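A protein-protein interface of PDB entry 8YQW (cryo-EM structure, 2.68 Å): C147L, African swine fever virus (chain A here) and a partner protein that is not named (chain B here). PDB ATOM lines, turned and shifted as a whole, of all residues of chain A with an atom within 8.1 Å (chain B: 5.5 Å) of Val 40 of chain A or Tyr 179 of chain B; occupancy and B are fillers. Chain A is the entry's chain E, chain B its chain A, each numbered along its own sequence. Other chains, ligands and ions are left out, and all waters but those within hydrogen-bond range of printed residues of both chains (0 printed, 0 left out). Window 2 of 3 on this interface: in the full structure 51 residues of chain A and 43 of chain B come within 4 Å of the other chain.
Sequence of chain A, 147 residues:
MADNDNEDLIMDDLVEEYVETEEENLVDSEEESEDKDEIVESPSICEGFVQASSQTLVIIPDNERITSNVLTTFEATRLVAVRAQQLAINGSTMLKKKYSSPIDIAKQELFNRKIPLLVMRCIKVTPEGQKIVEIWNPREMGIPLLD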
ATOM      1  N   ILE A  39       8.611   6.052  14.803  1.00  0.00           N
ATOM      2  CA  ILE A  39       8.195   5.640  13.468  1.00  0.00           C
ATOM      3  C   ILE A  39       6.735   6.001  13.224  1.00  0.00           C
ATOM      4  O   ILE A  39       5.919   5.993  14.145  1.00  0.00           O
ATOM      5  CB  ILE A  39       8.424   4.135  13.254  1.00  0.00           C
ATOM      6  CG1 ILE A  39       7.697   3.327  14.329  1.00  0.00           C
ATOM      7  CG2 ILE A  39       9.909   3.814  13.251  1.00  0.00           C
ATOM      8  CD1 ILE A  39       7.642   1.848  14.046  1.00  0.00           C
ATOM      9  N   VAL A  40       6.412   6.325  11.974  1.00  0.00           N
ATOM     10  CA  VAL A  40       5.052   6.682  11.584  1.00  0.00           C
ATOM     11  C   VAL A  40       4.404   5.427  11.009  1.00  0.00           C
ATOM     12  O   VAL A  40       4.675   5.034   9.873  1.00  0.00           O
ATOM     13  CB  VAL A  40       5.032   7.840  10.588  1.00  0.00           C
ATOM     14  CG1 VAL A  40       3.602   8.184  10.230  1.00  0.00           C
ATOM     15  CG2 VAL A  40       5.751   9.049  11.167  1.00  0.00           C
ATOM     16  N   GLU A  41       3.543   4.800  11.799  1.00  0.00           N
ATOM     17  CA  GLU A  41       2.963   3.511  11.460  1.00  0.00           C
ATOM     18  C   GLU A  41       1.623   3.689  10.745  1.00  0.00           C
ATOM     19  O   GLU A  41       1.267   4.782  10.297  1.00  0.00           O
ATOM     20  CB  GLU A  41       2.845   2.659  12.719  1.00  0.00           C
ATOM     21  CG  GLU A  41       2.018   3.298  13.814  1.00  0.00           C
ATOM     22  CD  GLU A  41       2.098   2.527  15.112  1.00  0.00           C
ATOM     23  OE1 GLU A  41       2.770   1.475  15.135  1.00  0.00           O
ATOM     24  OE2 GLU A  41       1.509   2.983  16.113  1.00  0.00           O
ATOM     25  N   SER A  42       0.873   2.596  10.628  1.00  0.00           N
ATOM     26  CA  SER A  42      -0.363   2.579   9.868  1.00  0.00           C
ATOM     27  C   SER A  42      -1.406   3.495  10.505  1.00  0.00           C
ATOM     28  O   SER A  42      -1.366   3.753  11.709  1.00  0.00           O
ATOM     29  CB  SER A  42      -0.896   1.151   9.783  1.00  0.00           C
ATOM     30  OG  SER A  42       0.058   0.289   9.187  1.00  0.00           O
ATOM     31  N   PRO A  43      -2.341   4.016   9.706  1.00  0.00           N
ATOM     32  CA  PRO A  43      -3.380   4.889  10.265  1.00  0.00           C
ATOM     33  C   PRO A  43      -4.228   4.166  11.299  1.00  0.00           C
ATOM     34  O   PRO A  43      -4.546   2.982  11.160  1.00  0.00           O
ATOM     35  CB  PRO A  43      -4.210   5.287   9.038  1.00  0.00           C
ATOM     36  CG  PRO A  43      -3.926   4.230   8.024  1.00  0.00           C
ATOM     37  CD  PRO A  43      -2.501   3.834   8.254  1.00  0.00           C
ATOM     38  N   GLU A  47      -7.604   8.813  14.326  1.00  0.00           N
ATOM     39  CA  GLU A  47      -7.856   9.697  13.200  1.00  0.00           C
ATOM     40  C   GLU A  47      -8.731   8.983  12.172  1.00  0.00           C
ATOM     41  O   GLU A  47      -9.129   7.830  12.347  1.00  0.00           O
ATOM     42  CB  GLU A  47      -6.551  10.178  12.559  1.00  0.00           C
ATOM     43  CG  GLU A  47      -5.738   9.111  11.847  1.00  0.00           C
ATOM     44  CD  GLU A  47      -4.551   8.643  12.663  1.00  0.00           C
ATOM     45  OE1 GLU A  47      -4.540   8.884  13.884  1.00  0.00           O
ATOM     46  OE2 GLU A  47      -3.625   8.041  12.080  1.00  0.00           O
ATOM     47  N   VAL B 177       5.931  -0.504   0.022  1.00  0.00           N
ATOM     48  CA  VAL B 177       6.270   0.780   0.625  1.00  0.00           C
ATOM     49  C   VAL B 177       5.576   0.898   1.974  1.00  0.00           C
ATOM     50  O   VAL B 177       4.391   0.573   2.107  1.00  0.00           O
ATOM     51  CB  VAL B 177       5.867   1.938  -0.300  1.00  0.00           C
ATOM     52  CG1 VAL B 177       6.352   3.264   0.261  1.00  0.00           C
ATOM     53  CG2 VAL B 177       6.407   1.715  -1.689  1.00  0.00           C
ATOM     54  N   THR B 178       6.310   1.363   2.979  1.00  0.00           N
ATOM     55  CA  THR B 178       5.738   1.531   4.302  1.00  0.00           C
ATOM     56  C   THR B 178       5.086   2.904   4.433  1.00  0.00           C
ATOM     57  O   THR B 178       5.361   3.828   3.664  1.00  0.00           O
ATOM     58  CB  THR B 178       6.808   1.351   5.379  1.00  0.00           C
ATOM     59  OG1 THR B 178       7.797   2.379   5.248  1.00  0.00           O
ATOM     60  CG2 THR B 178       7.477  -0.003   5.234  1.00  0.00           C
ATOM     61  N   TYR B 179       4.198   3.027   5.423  1.00  0.00           N
ATOM     62  CA  TYR B 179       3.539   4.306   5.664  1.00  0.00           C
ATOM     63  C   TYR B 179       4.521   5.359   6.153  1.00  0.00           C
ATOM     64  O   TYR B 179       4.295   6.558   5.951  1.00  0.00           O
ATOM     65  CB  TYR B 179       2.402   4.140   6.669  1.00  0.00           C
ATOM     66  CG  TYR B 179       1.105   3.681   6.047  1.00  0.00           C
ATOM     67  CD1 TYR B 179       0.414   4.490   5.160  1.00  0.00           C
ATOM     68  CD2 TYR B 179       0.571   2.438   6.352  1.00  0.00           C
ATOM     69  CE1 TYR B 179      -0.770   4.074   4.591  1.00  0.00           C
ATOM     70  CE2 TYR B 179      -0.611   2.013   5.788  1.00  0.00           C
ATOM     71  CZ  TYR B 179      -1.278   2.833   4.910  1.00  0.00           C
ATOM     72  OH  TYR B 179      -2.459   2.410   4.348  1.00  0.00           O
ATOM     73  N   ASP B 180       5.608   4.935   6.799  1.00  0.00           N
ATOM     74  CA  ASP B 180       6.635   5.879   7.219  1.00  0.00           C
ATOM     75  C   ASP B 180       7.256   6.577   6.018  1.00  0.00           C
ATOM     76  O   ASP B 180       7.499   7.789   6.050  1.00  0.00           O
ATOM     77  CB  ASP B 180       7.704   5.153   8.032  1.00  0.00           C
ATOM     78  CG  ASP B 180       8.348   6.040   9.072  1.00  0.00           C
ATOM     79  OD1 ASP B 180       8.884   7.102   8.701  1.00  0.00           O
ATOM     80  OD2 ASP B 180       8.325   5.672  10.264  1.00  0.00           O
ATOM     81  N   THR B 181       7.519   5.827   4.946  1.00  0.00           N
ATOM     82  CA  THR B 181       8.055   6.427   3.730  1.00  0.00           C
ATOM     83  C   THR B 181       7.071   7.423   3.132  1.00  0.00           C
ATOM     84  O   THR B 181       7.467   8.504   2.682  1.00  0.00           O
ATOM     85  CB  THR B 181       8.395   5.338   2.712  1.00  0.00           C
ATOM     86  OG1 THR B 181       9.385   4.460   3.261  1.00  0.00           O
ATOM     87  CG2 THR B 181       8.926   5.947   1.430  1.00  0.00           C
ATOM     88  N   VAL B 182       5.783   7.077   3.123  1.00  0.00           N
ATOM     89  CA  VAL B 182       4.772   7.959   2.547  1.00  0.00           C
ATOM     90  C   VAL B 182       4.682   9.256   3.339  1.00  0.00           C
ATOM     91  O   VAL B 182       4.640  10.351   2.770  1.00  0.00           O
ATOM     92  CB  VAL B 182       3.412   7.243   2.484  1.00  0.00           C
ATOM     93  CG1 VAL B 182       2.366   8.148   1.868  1.00  0.00           C
ATOM     94  CG2 VAL B 182       3.534   5.955   1.699  1.00  0.00           C
ATOM     95  N   VAL B 183       4.651   9.149   4.668  1.00  0.00           N
ATOM     96  CA  VAL B 183       4.518  10.340   5.500  1.00  0.00           C
ATOM     97  C   VAL B 183       5.771  11.203   5.417  1.00  0.00           C
ATOM     98  O   VAL B 183       5.684  12.430   5.290  1.00  0.00           O
ATOM     99  CB  VAL B 183       4.192   9.939   6.949  1.00  0.00           C
ATOM    100  CG1 VAL B 183       4.432  11.104   7.889  1.00  0.00           C
ATOM    101  CG2 VAL B 183       2.754   9.469   7.041  1.00  0.00           C
ATOM    102  N   LYS B 184       6.953  10.588   5.475  1.00  0.00           N
ATOM    103  CA  LYS B 184       8.182  11.371   5.422  1.00  0.00           C
ATOM    104  C   LYS B 184       8.461  11.942   4.039  1.00  0.00           C
ATOM    105  O   LYS B 184       9.342  12.799   3.911  1.00  0.00           O
ATOM    106  CB  LYS B 184       9.374  10.529   5.883  1.00  0.00           C
ATOM    107  CG  LYS B 184       9.336  10.154   7.354  1.00  0.00           C
ATOM    108  CD  LYS B 184      10.726   9.848   7.889  1.00  0.00           C
ATOM    109  CE  LYS B 184      11.272   8.551   7.320  1.00  0.00           C
ATOM    110  NZ  LYS B 184      12.571   8.168   7.931  1.00  0.00           N
ATOM    111  N   LYS B 189      -1.416   9.714   4.680  1.00  0.00           N
ATOM    112  CA  LYS B 189      -1.659   8.284   4.816  1.00  0.00           C
ATOM    113  C   LYS B 189      -2.753   7.790   3.881  1.00  0.00           C
ATOM    114  O   LYS B 189      -2.837   6.585   3.628  1.00  0.00           O
ATOM    115  CB  LYS B 189      -2.018   7.944   6.262  1.00  0.00           C
ATOM    116  CG  LYS B 189      -0.892   8.185   7.248  1.00  0.00           C
ATOM    117  CD  LYS B 189      -1.302   7.809   8.659  1.00  0.00           C
ATOM    118  CE  LYS B 189      -0.086   7.612   9.550  1.00  0.00           C
ATOM    119  NZ  LYS B 189       0.307   8.869  10.245  1.00  0.00           N
ATOM    120  N   HIS B 192      -1.274   6.629  -0.077  1.00  0.00           N
ATOM    121  CA  HIS B 192      -0.322   5.544  -0.248  1.00  0.00           C
ATOM    122  C   HIS B 192      -0.307   5.108  -1.710  1.00  0.00           C
ATOM    123  O   HIS B 192      -1.367   5.018  -2.342  1.00  0.00           O
ATOM    124  CB  HIS B 192      -0.685   4.364   0.654  1.00  0.00           C
ATOM    125  CG  HIS B 192       0.431   3.389   0.855  1.00  0.00           C
ATOM    126  ND1 HIS B 192       0.825   2.497  -0.118  1.00  0.00           N
ATOM    127  CD2 HIS B 192       1.234   3.161   1.920  1.00  0.00           C
ATOM    128  CE1 HIS B 192       1.825   1.764   0.338  1.00  0.00           C
ATOM    129  NE2 HIS B 192       2.093   2.148   1.572  1.00  0.00           N
ATOM    130  N   GLU B 194      -0.126   2.366  -3.156  1.00  0.00           N
ATOM    131  CA  GLU B 194      -0.834   1.137  -3.500  1.00  0.00           C
ATOM    132  C   GLU B 194      -2.186   1.420  -4.139  1.00  0.00           C
ATOM    133  O   GLU B 194      -2.652   0.636  -4.973  1.00  0.00           O
ATOM    134  CB  GLU B 194      -1.018   0.263  -2.259  1.00  0.00           C
ATOM    135  CG  GLU B 194      -1.857   0.900  -1.168  1.00  0.00           C
ATOM    136  CD  GLU B 194      -2.193  -0.066  -0.053  1.00  0.00           C
ATOM    137  OE1 GLU B 194      -1.888  -1.268  -0.194  1.00  0.00           O
ATOM    138  OE2 GLU B 194      -2.758   0.377   0.968  1.00  0.00           O
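Asp 180 of chain B touches Ile 39 of chain A. Val 40 of chain A touches Tyr 179 of chain B. Val 40 of chain A touches Val 183 of chain B. CG1 of Val 40 of chain A touches NZ of Lys 189 of chain B, 3.4 Å away. Tyr 179 of chain B touches Glu 41 of chain A. O of Glu 41 of chain A touches CE of Lys 189 of chain B, 3.2 Å away. OG of Ser 42 of chain A touches CD2 of Tyr 179 of chain B, 3.6 Å away. CE2 of Tyr 179 of chain B touches CD of Pro 43 of chain A, 3.6 Å away. CB of Pro 43 of chain A touches CD of Lys 189 of chain B, at 3.9 Å.
The side-chain carboxylate of Asp 180 of chain B lies within hydrogen-bond range of the backbone NH of Val 40 of chain A (2.6 Å).
The side-chain amino group (NZ) of Lys 184 of chain B is in salt-bridge range of the side-chain carboxylate (OD1) of Asp 180 of chain B (3.9 Å).
Printed residues of chain B that touch a printed residue of chain A: Tyr 179, Asp 180, Val 183 and Lys 189. Hydrophobic or aromatic side chains of chain B that line the printed part of chain A: Tyr 179 and Val 183. Hydrophobic or aromatic side chains of chain A within 4 Å of the printed part of chain B: Ile 39, Val 40 and Pro 43.
Val 40 of chain A touches four residues of chain B. Printed residues of chain B within 4 Å of Pro 43 of chain A: Tyr 179 (3.6 Å) and Lys 189 (3.9 Å). Val 177 of chain B touches none of the printed residues of chain A. Tyr 179 of chain B touches just these residues of chain A: Val 40, Glu 41, Ser 42 and Pro 43. Printed residues of chain A within 4 Å of Asp 180 of chain B: Ile 39 and Val 40. Val 182 of chain B touches none of the printed residues of chain A. Of the printed residues of chain A, Val 183 of chain B touches Val 40 (3.5 Å). Printed residues of chain A within 4 Å of Lys 189 of chain B: Val 40, Glu 41 and Pro 43. The nearest residue of chain B that does not touch Val 40 of chain A is Lys 184 of chain B (5.3 Å). The nearest residue of chain A that does not touch Tyr 179 of chain B is Ile 39 of chain A (7.4 Å).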
